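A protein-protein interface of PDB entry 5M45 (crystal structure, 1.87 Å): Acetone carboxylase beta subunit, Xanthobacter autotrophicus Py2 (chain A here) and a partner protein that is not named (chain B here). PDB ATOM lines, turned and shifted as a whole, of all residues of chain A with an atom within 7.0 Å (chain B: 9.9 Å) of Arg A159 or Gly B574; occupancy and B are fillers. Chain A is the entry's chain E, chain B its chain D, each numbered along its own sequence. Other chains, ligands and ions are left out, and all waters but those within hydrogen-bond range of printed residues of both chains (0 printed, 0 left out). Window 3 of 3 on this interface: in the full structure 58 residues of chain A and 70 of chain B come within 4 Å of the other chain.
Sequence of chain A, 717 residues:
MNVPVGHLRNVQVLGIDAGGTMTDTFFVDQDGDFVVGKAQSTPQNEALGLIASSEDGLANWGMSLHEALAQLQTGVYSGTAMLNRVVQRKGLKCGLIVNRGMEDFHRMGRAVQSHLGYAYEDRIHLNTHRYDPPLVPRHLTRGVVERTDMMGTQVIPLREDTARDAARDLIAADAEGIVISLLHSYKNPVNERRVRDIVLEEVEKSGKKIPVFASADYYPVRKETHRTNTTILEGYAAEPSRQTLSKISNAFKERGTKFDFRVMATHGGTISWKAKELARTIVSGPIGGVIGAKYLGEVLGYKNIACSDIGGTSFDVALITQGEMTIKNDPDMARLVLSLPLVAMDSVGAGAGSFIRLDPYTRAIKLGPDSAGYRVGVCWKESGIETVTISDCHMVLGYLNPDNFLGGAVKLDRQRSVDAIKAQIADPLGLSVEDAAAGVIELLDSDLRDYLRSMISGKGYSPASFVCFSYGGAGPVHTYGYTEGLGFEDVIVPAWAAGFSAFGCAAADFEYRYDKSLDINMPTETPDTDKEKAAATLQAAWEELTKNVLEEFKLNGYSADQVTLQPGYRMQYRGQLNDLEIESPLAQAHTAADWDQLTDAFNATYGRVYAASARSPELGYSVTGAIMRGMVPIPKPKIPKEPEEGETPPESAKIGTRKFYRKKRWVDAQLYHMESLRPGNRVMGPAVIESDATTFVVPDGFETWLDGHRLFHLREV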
ATOM      1  N   VAL A 144     -12.740   9.862 -23.498  1.00  0.00           N
ATOM      2  CA  VAL A 144     -13.036  11.289 -23.281  1.00  0.00           C
ATOM      3  C   VAL A 144     -12.027  11.911 -22.313  1.00  0.00           C
ATOM      4  O   VAL A 144     -11.545  11.216 -21.391  1.00  0.00           O
ATOM      5  CB  VAL A 144     -14.470  11.524 -22.750  1.00  0.00           C
ATOM      6  CG1 VAL A 144     -15.497  10.940 -23.717  1.00  0.00           C
ATOM      7  CG2 VAL A 144     -14.683  10.892 -21.364  1.00  0.00           C
ATOM      8  N   VAL A 145     -11.694  13.190 -22.503  1.00  0.00           N
ATOM      9  CA  VAL A 145     -10.722  13.857 -21.616  1.00  0.00           C
ATOM     10  C   VAL A 145     -11.453  14.420 -20.371  1.00  0.00           C
ATOM     11  O   VAL A 145     -12.314  15.326 -20.468  1.00  0.00           O
ATOM     12  CB  VAL A 145      -9.966  14.983 -22.337  1.00  0.00           C
ATOM     13  CG1 VAL A 145      -9.009  15.687 -21.380  1.00  0.00           C
ATOM     14  CG2 VAL A 145      -9.217  14.419 -23.531  1.00  0.00           C
ATOM     15  N   GLU A 146     -11.083  13.837 -19.219  1.00  0.00           N
ATOM     16  CA  GLU A 146     -11.719  14.045 -17.926  1.00  0.00           C
ATOM     17  C   GLU A 146     -10.901  13.335 -16.847  1.00  0.00           C
ATOM     18  O   GLU A 146     -10.313  12.276 -17.136  1.00  0.00           O
ATOM     19  CB  GLU A 146     -13.101  13.403 -17.962  1.00  0.00           C
ATOM     20  CG  GLU A 146     -13.946  13.548 -16.734  1.00  0.00           C
ATOM     21  CD  GLU A 146     -13.804  12.487 -15.618  1.00  0.00           C
ATOM     22  OE1 GLU A 146     -13.285  11.352 -15.781  1.00  0.00           O
ATOM     23  OE2 GLU A 146     -14.281  12.859 -14.505  1.00  0.00           O
ATOM     24  N   ILE A 156      -9.334  17.319 -13.845  1.00  0.00           N
ATOM     25  CA  ILE A 156      -9.418  17.728 -15.256  1.00  0.00           C
ATOM     26  C   ILE A 156     -10.922  17.810 -15.612  1.00  0.00           C
ATOM     27  O   ILE A 156     -11.587  16.779 -15.729  1.00  0.00           O
ATOM     28  CB  ILE A 156      -8.696  16.740 -16.196  1.00  0.00           C
ATOM     29  CG1 ILE A 156      -7.187  16.721 -15.879  1.00  0.00           C
ATOM     30  CG2 ILE A 156      -8.928  17.102 -17.658  1.00  0.00           C
ATOM     31  CD1 ILE A 156      -6.370  15.655 -16.588  1.00  0.00           C
ATOM     32  N   PRO A 157     -11.468  19.031 -15.772  1.00  0.00           N
ATOM     33  CA  PRO A 157     -12.869  19.164 -16.187  1.00  0.00           C
ATOM     34  C   PRO A 157     -13.175  18.415 -17.480  1.00  0.00           C
ATOM     35  O   PRO A 157     -12.338  18.373 -18.375  1.00  0.00           O
ATOM     36  CB  PRO A 157     -13.034  20.705 -16.387  1.00  0.00           C
ATOM     37  CG  PRO A 157     -12.005  21.310 -15.475  1.00  0.00           C
ATOM     38  CD  PRO A 157     -10.832  20.342 -15.545  1.00  0.00           C
ATOM     39  N   LEU A 158     -14.374  17.841 -17.579  1.00  0.00           N
ATOM     40  CA  LEU A 158     -14.818  17.149 -18.812  1.00  0.00           C
ATOM     41  C   LEU A 158     -14.747  18.068 -20.007  1.00  0.00           C
ATOM     42  O   LEU A 158     -15.305  19.180 -19.959  1.00  0.00           O
ATOM     43  CB  LEU A 158     -16.264  16.642 -18.693  1.00  0.00           C
ATOM     44  CG  LEU A 158     -16.858  15.950 -19.946  1.00  0.00           C
ATOM     45  CD1 LEU A 158     -16.081  14.668 -20.304  1.00  0.00           C
ATOM     46  CD2 LEU A 158     -18.317  15.673 -19.728  1.00  0.00           C
ATOM     47  N   ARG A 159     -14.053  17.624 -21.066  1.00  0.00           N
ATOM     48  CA  ARG A 159     -14.027  18.352 -22.353  1.00  0.00           C
ATOM     49  C   ARG A 159     -15.120  17.728 -23.242  1.00  0.00           C
ATOM     50  O   ARG A 159     -14.974  16.619 -23.787  1.00  0.00           O
ATOM     51  CB  ARG A 159     -12.632  18.304 -22.972  1.00  0.00           C
ATOM     52  CG  ARG A 159     -11.611  18.956 -22.037  1.00  0.00           C
ATOM     53  CD  ARG A 159     -10.216  18.996 -22.588  1.00  0.00           C
ATOM     54  NE  ARG A 159      -9.288  19.742 -21.715  1.00  0.00           N
ATOM     55  CZ  ARG A 159      -8.022  19.996 -22.035  1.00  0.00           C
ATOM     56  NH1 ARG A 159      -7.517  19.519 -23.168  1.00  0.00           N
ATOM     57  NH2 ARG A 159      -7.232  20.707 -21.219  1.00  0.00           N
ATOM     58  N   GLU A 160     -16.236  18.452 -23.343  1.00  0.00           N
ATOM     59  CA  GLU A 160     -17.472  17.902 -23.942  1.00  0.00           C
ATOM     60  C   GLU A 160     -17.352  17.548 -25.419  1.00  0.00           C
ATOM     61  O   GLU A 160     -17.963  16.586 -25.861  1.00  0.00           O
ATOM     62  CB  GLU A 160     -18.659  18.853 -23.722  1.00  0.00           C
ATOM     63  CG  GLU A 160     -19.008  19.043 -22.255  1.00  0.00           C
ATOM     64  CD  GLU A 160     -20.397  19.614 -22.002  1.00  0.00           C
ATOM     65  OE1 GLU A 160     -21.054  20.015 -22.983  1.00  0.00           O
ATOM     66  OE2 GLU A 160     -20.820  19.639 -20.822  1.00  0.00           O
ATOM     67  N   ASP A 161     -16.568  18.324 -26.172  1.00  0.00           N
ATOM     68  CA  ASP A 161     -16.284  18.003 -27.593  1.00  0.00           C
ATOM     69  C   ASP A 161     -15.677  16.580 -27.779  1.00  0.00           C
ATOM     70  O   ASP A 161     -15.980  15.904 -28.762  1.00  0.00           O
ATOM     71  CB  ASP A 161     -15.410  19.082 -28.261  1.00  0.00           C
ATOM     72  CG  ASP A 161     -14.033  19.301 -27.550  1.00  0.00           C
ATOM     73  OD1 ASP A 161     -13.922  19.241 -26.289  1.00  0.00           O
ATOM     74  OD2 ASP A 161     -13.021  19.569 -28.245  1.00  0.00           O
ATOM     75  N   THR A 162     -14.847  16.120 -26.828  1.00  0.00           N
ATOM     76  CA  THR A 162     -14.239  14.785 -26.922  1.00  0.00           C
ATOM     77  C   THR A 162     -15.317  13.662 -26.692  1.00  0.00           C
ATOM     78  O   THR A 162     -15.246  12.586 -27.282  1.00  0.00           O
ATOM     79  CB  THR A 162     -13.026  14.604 -25.982  1.00  0.00           C
ATOM     80  OG1 THR A 162     -13.437  14.491 -24.597  1.00  0.00           O
ATOM     81  CG2 THR A 162     -12.015  15.717 -26.173  1.00  0.00           C
ATOM     82  N   ALA A 163     -16.305  13.948 -25.862  1.00  0.00           N
ATOM     83  CA  ALA A 163     -17.482  13.059 -25.683  1.00  0.00           C
ATOM     84  C   ALA A 163     -18.362  12.960 -26.939  1.00  0.00           C
ATOM     85  O   ALA A 163     -18.845  11.871 -27.289  1.00  0.00           O
ATOM     86  CB  ALA A 163     -18.312  13.498 -24.484  1.00  0.00           C
ATOM     87  N   ARG A 164     -18.558  14.085 -27.614  1.00  0.00           N
ATOM     88  CA  ARG A 164     -19.287  14.102 -28.888  1.00  0.00           C
ATOM     89  C   ARG A 164     -18.617  13.338 -29.994  1.00  0.00           C
ATOM     90  O   ARG A 164     -19.299  12.597 -30.704  1.00  0.00           O
ATOM     91  CB  ARG A 164     -19.546  15.521 -29.412  1.00  0.00           C
ATOM     92  CG  ARG A 164     -20.799  16.040 -28.872  1.00  0.00           C
ATOM     93  CD  ARG A 164     -21.267  17.359 -29.463  1.00  0.00           C
ATOM     94  NE  ARG A 164     -21.975  17.966 -28.345  1.00  0.00           N
ATOM     95  CZ  ARG A 164     -23.184  17.642 -27.891  1.00  0.00           C
ATOM     96  NH1 ARG A 164     -23.588  18.266 -26.783  1.00  0.00           N
ATOM     97  NH2 ARG A 164     -23.972  16.717 -28.487  1.00  0.00           N
ATOM     98  N   VAL A 195     -21.589  12.718 -19.946  1.00  0.00           N
ATOM     99  CA  VAL A 195     -21.154  11.948 -21.148  1.00  0.00           C
ATOM    100  C   VAL A 195     -22.309  11.080 -21.670  1.00  0.00           C
ATOM    101  O   VAL A 195     -22.561  11.051 -22.866  1.00  0.00           O
ATOM    102  CB  VAL A 195     -19.899  11.076 -20.861  1.00  0.00           C
ATOM    103  CG1 VAL A 195     -19.575  10.153 -22.029  1.00  0.00           C
ATOM    104  CG2 VAL A 195     -18.693  11.935 -20.535  1.00  0.00           C
ATOM    105  N   ILE A 198     -24.809  13.369 -23.477  1.00  0.00           N
ATOM    106  CA  ILE A 198     -24.238  13.740 -24.784  1.00  0.00           C
ATOM    107  C   ILE A 198     -24.288  12.559 -25.773  1.00  0.00           C
ATOM    108  O   ILE A 198     -24.651  12.752 -26.932  1.00  0.00           O
ATOM    109  CB  ILE A 198     -22.789  14.266 -24.661  1.00  0.00           C
ATOM    110  CG1 ILE A 198     -22.778  15.648 -23.978  1.00  0.00           C
ATOM    111  CG2 ILE A 198     -22.100  14.346 -26.030  1.00  0.00           C
ATOM    112  CD1 ILE A 198     -21.399  15.986 -23.408  1.00  0.00           C
ATOM    113  N   ASN B 566       3.496  23.393 -15.468  1.00  0.00           N
ATOM    114  CA  ASN B 566       2.425  24.370 -15.693  1.00  0.00           C
ATOM    115  C   ASN B 566       1.081  23.698 -16.051  1.00  0.00           C
ATOM    116  O   ASN B 566       0.201  24.338 -16.655  1.00  0.00           O
ATOM    117  CB  ASN B 566       2.861  25.394 -16.774  1.00  0.00           C
ATOM    118  CG  ASN B 566       2.029  26.672 -16.773  1.00  0.00           C
ATOM    119  OD1 ASN B 566       1.644  27.190 -15.725  1.00  0.00           O
ATOM    120  ND2 ASN B 566       1.758  27.197 -17.943  1.00  0.00           N
ATOM    121  N   LEU B 567       0.893  22.429 -15.675  1.00  0.00           N
ATOM    122  CA  LEU B 567      -0.327  21.709 -16.083  1.00  0.00           C
ATOM    123  C   LEU B 567      -1.619  22.291 -15.485  1.00  0.00           C
ATOM    124  O   LEU B 567      -2.655  22.170 -16.100  1.00  0.00           O
ATOM    125  CB  LEU B 567      -0.239  20.192 -15.809  1.00  0.00           C
ATOM    126  CG  LEU B 567       0.450  19.404 -16.937  1.00  0.00           C
ATOM    127  CD1 LEU B 567       0.866  18.008 -16.474  1.00  0.00           C
ATOM    128  CD2 LEU B 567      -0.483  19.282 -18.135  1.00  0.00           C
ATOM    129  N   LYS B 568      -1.572  22.905 -14.305  1.00  0.00           N
ATOM    130  CA  LYS B 568      -2.792  23.516 -13.748  1.00  0.00           C
ATOM    131  C   LYS B 568      -3.405  24.511 -14.741  1.00  0.00           C
ATOM    132  O   LYS B 568      -4.614  24.447 -15.039  1.00  0.00           O
ATOM    133  CB  LYS B 568      -2.534  24.184 -12.411  1.00  0.00           C
ATOM    134  CG  LYS B 568      -3.822  24.682 -11.757  1.00  0.00           C
ATOM    135  CD  LYS B 568      -3.565  25.322 -10.418  1.00  0.00           C
ATOM    136  CE  LYS B 568      -4.807  25.250  -9.563  1.00  0.00           C
ATOM    137  NZ  LYS B 568      -5.033  26.564  -8.907  1.00  0.00           N
ATOM    138  N   GLU B 569      -2.561  25.406 -15.272  1.00  0.00           N
ATOM    139  CA  GLU B 569      -3.007  26.408 -16.248  1.00  0.00           C
ATOM    140  C   GLU B 569      -3.330  25.780 -17.616  1.00  0.00           C
ATOM    141  O   GLU B 569      -4.294  26.206 -18.263  1.00  0.00           O
ATOM    142  CB  GLU B 569      -1.918  27.479 -16.369  1.00  0.00           C
ATOM    143  CG  GLU B 569      -2.217  28.728 -17.216  1.00  0.00           C
ATOM    144  CD  GLU B 569      -1.025  29.720 -17.158  1.00  0.00           C
ATOM    145  OE1 GLU B 569      -0.243  29.842 -18.165  1.00  0.00           O
ATOM    146  OE2 GLU B 569      -0.816  30.333 -16.056  1.00  0.00           O
ATOM    147  N   LEU B 570      -2.544  24.785 -18.057  1.00  0.00           N
ATOM    148  CA  LEU B 570      -2.817  24.107 -19.326  1.00  0.00           C
ATOM    149  C   LEU B 570      -4.157  23.355 -19.307  1.00  0.00           C
ATOM    150  O   LEU B 570      -4.914  23.414 -20.277  1.00  0.00           O
ATOM    151  CB  LEU B 570      -1.670  23.166 -19.742  1.00  0.00           C
ATOM    152  CG  LEU B 570      -0.309  23.797 -20.001  1.00  0.00           C
ATOM    153  CD1 LEU B 570       0.751  22.705 -20.038  1.00  0.00           C
ATOM    154  CD2 LEU B 570      -0.256  24.643 -21.276  1.00  0.00           C
ATOM    155  N   ILE B 571      -4.467  22.698 -18.193  1.00  0.00           N
ATOM    156  CA  ILE B 571      -5.754  22.036 -18.021  1.00  0.00           C
ATOM    157  C   ILE B 571      -6.900  23.073 -18.093  1.00  0.00           C
ATOM    158  O   ILE B 571      -7.849  22.901 -18.877  1.00  0.00           O
ATOM    159  CB  ILE B 571      -5.805  21.235 -16.693  1.00  0.00           C
ATOM    160  CG1 ILE B 571      -4.886  20.005 -16.762  1.00  0.00           C
ATOM    161  CG2 ILE B 571      -7.223  20.817 -16.358  1.00  0.00           C
ATOM    162  CD1 ILE B 571      -4.483  19.500 -15.384  1.00  0.00           C
ATOM    163  N   ALA B 572      -6.788  24.128 -17.294  1.00  0.00           N
ATOM    164  CA  ALA B 572      -7.798  25.184 -17.233  1.00  0.00           C
ATOM    165  C   ALA B 572      -8.012  25.930 -18.562  1.00  0.00           C
ATOM    166  O   ALA B 572      -9.119  26.320 -18.849  1.00  0.00           O
ATOM    167  CB  ALA B 572      -7.451  26.183 -16.121  1.00  0.00           C
ATOM    168  N   SER B 573      -6.987  26.113 -19.362  1.00  0.00           N
ATOM    169  CA  SER B 573      -7.104  26.897 -20.608  1.00  0.00           C
ATOM    170  C   SER B 573      -7.597  26.053 -21.807  1.00  0.00           C
ATOM    171  O   SER B 573      -7.822  26.591 -22.860  1.00  0.00           O
ATOM    172  CB  SER B 573      -5.783  27.578 -20.940  1.00  0.00           C
ATOM    173  OG  SER B 573      -4.796  26.621 -21.294  1.00  0.00           O
ATOM    174  N   GLY B 574      -7.783  24.747 -21.632  1.00  0.00           N
ATOM    175  CA  GLY B 574      -8.165  23.860 -22.732  1.00  0.00           C
ATOM    176  C   GLY B 574      -7.033  23.452 -23.666  1.00  0.00           C
ATOM    177  O   GLY B 574      -7.307  22.910 -24.738  1.00  0.00           O
ATOM    178  N   ALA B 575      -5.782  23.671 -23.279  1.00  0.00           N
ATOM    179  CA  ALA B 575      -4.619  23.263 -24.087  1.00  0.00           C
ATOM    180  C   ALA B 575      -4.430  21.737 -24.131  1.00  0.00           C
ATOM    181  O   ALA B 575      -4.953  21.044 -23.273  1.00  0.00           O
ATOM    182  CB  ALA B 575      -3.343  23.916 -23.535  1.00  0.00           C
ATOM    183  N   GLU B 576      -3.668  21.235 -25.105  1.00  0.00           N
ATOM    184  CA  GLU B 576      -3.381  19.784 -25.175  1.00  0.00           C
ATOM    185  C   GLU B 576      -2.636  19.364 -23.914  1.00  0.00           C
ATOM    186  O   GLU B 576      -1.738  20.059 -23.462  1.00  0.00           O
ATOM    187  CB  GLU B 576      -2.425  19.348 -26.285  1.00  0.00           C
ATOM    188  CG  GLU B 576      -2.675  19.715 -27.720  1.00  0.00           C
ATOM    189  CD  GLU B 576      -1.548  19.138 -28.610  1.00  0.00           C
ATOM    190  OE1 GLU B 576      -1.720  17.938 -28.987  1.00  0.00           O
ATOM    191  OE2 GLU B 576      -0.494  19.862 -28.855  1.00  0.00           O
ATOM    192  N   ILE B 577      -3.009  18.221 -23.370  1.00  0.00           N
ATOM    193  CA  ILE B 577      -2.317  17.655 -22.219  1.00  0.00           C
ATOM    194  C   ILE B 577      -1.822  16.213 -22.471  1.00  0.00           C
ATOM    195  O   ILE B 577      -2.463  15.458 -23.230  1.00  0.00           O
ATOM    196  CB  ILE B 577      -3.158  17.760 -20.947  1.00  0.00           C
ATOM    197  CG1 ILE B 577      -4.491  17.081 -21.073  1.00  0.00           C
ATOM    198  CG2 ILE B 577      -3.376  19.241 -20.583  1.00  0.00           C
ATOM    199  CD1 ILE B 577      -5.386  17.375 -19.880  1.00  0.00           C
ATOM    200  N   PRO B 578      -0.657  15.856 -21.903  1.00  0.00           N
ATOM    201  CA  PRO B 578      -0.151  14.469 -22.067  1.00  0.00           C
ATOM    202  C   PRO B 578      -1.118  13.443 -21.472  1.00  0.00           C
ATOM    203  O   PRO B 578      -1.508  13.572 -20.306  1.00  0.00           O
ATOM    204  CB  PRO B 578       1.178  14.447 -21.286  1.00  0.00           C
ATOM    205  CG  PRO B 578       1.532  15.863 -21.136  1.00  0.00           C
ATOM    206  CD  PRO B 578       0.269  16.682 -21.134  1.00  0.00           C
ATOM    207  N   LEU B 579      -1.500  12.454 -22.275  1.00  0.00           N
ATOM    208  CA  LEU B 579      -2.327  11.317 -21.824  1.00  0.00           C
ATOM    209  C   LEU B 579      -1.825  10.028 -22.496  1.00  0.00           C
ATOM    210  O   LEU B 579      -1.118  10.070 -23.510  1.00  0.00           O
ATOM    211  CB  LEU B 579      -3.813  11.534 -22.157  1.00  0.00           C
ATOM    212  CG  LEU B 579      -4.493  12.830 -21.654  1.00  0.00           C
ATOM    213  CD1 LEU B 579      -5.791  13.152 -22.369  1.00  0.00           C
ATOM    214  CD2 LEU B 579      -4.755  12.730 -20.159  1.00  0.00           C
ATOM    215  N   MET B 593       4.263  19.502 -25.662  1.00  0.00           N
ATOM    216  CA  MET B 593       3.067  20.018 -24.973  1.00  0.00           C
ATOM    217  C   MET B 593       3.418  20.776 -23.670  1.00  0.00           C
ATOM    218  O   MET B 593       2.550  21.454 -23.111  1.00  0.00           O
ATOM    219  CB  MET B 593       2.112  18.877 -24.632  1.00  0.00           C
ATOM    220  CG  MET B 593       1.607  18.036 -25.815  1.00  0.00           C
ATOM    221  SD  MET B 593       0.564  16.672 -25.224  1.00  0.00           S
ATOM    222  CE  MET B 593       0.435  15.724 -26.757  1.00  0.00           C
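Of chain B, only Leu B570 (3.7 Å), Ile B571 (3.3 Å), Gly B574 (3.6 Å) and Ala B575 (3.0 Å) come within 4 Å of Arg A159. Of chain A, only Arg A159 comes within 4 Å of Gly B574. No residue of chain B comes within 4 Å of Leu A158. No residue of chain B comes within 4 Å of Asp A161. Thr A162 touches none of the printed residues of chain B. Of the printed residues of chain A, Ile B571 touches Ile A156 (3.9 Å), Pro A157 (3.7 Å) and Arg A159 (3.3 Å). Printed residues of chain B within 4 Å of Ile A156: Ile B571 (3.9 Å) and Ile B577 (3.8 Å). Met B593 touches none of the printed residues of chain A. Asn B566 touches none of the printed residues of chain A. The nearest residue of chain B that does not touch Arg A159 is Ile B577 (4.04 Å).
The guanidinium group of Arg A159 sits at hydrogen-bond distance from the backbone carbonyl oxygen of Ile B571, at 3.3 Å. The guanidinium group of Arg A159 lies within hydrogen-bond range of the backbone carbonyl oxygen of Ala B575, 3.0 Å away.
Of the 14 printed residues of chain A, 4 touch a printed residue of chain B. Printed residues of chain A that touch a printed residue of chain B: Val A145, Ile A156, Pro A157 and Arg A159. Hydrophobic or aromatic side chains of chain A that line the printed part of chain B: Val A145, Ile A156 and Pro A157.
Among the printed residues, merely in contact across the chains: Arg A159 with Gly B574, Arg A159 with Leu B570, Pro A157 with Ile B571, Val A145 with Leu B579, Ile A156 with Ile B577 and Ile A156 with Ile B571.
O of Leu B570 lies within hydrogen-bond range of OG of Ser B573 (3.4 Å). N of Ala B575 is in hydrogen-bond range of O of Leu B570, 3.1 Å away. The backbone carbonyl oxygen of Val A145 is in hydrogen-bond range of the backbone NH of Arg A159. N of Val A145 lies within hydrogen-bond range of OG1 of Thr A162 (3.0 Å). O of Arg A159 is in hydrogen-bond range of OG1 of Thr A162, 2.7 Å away.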
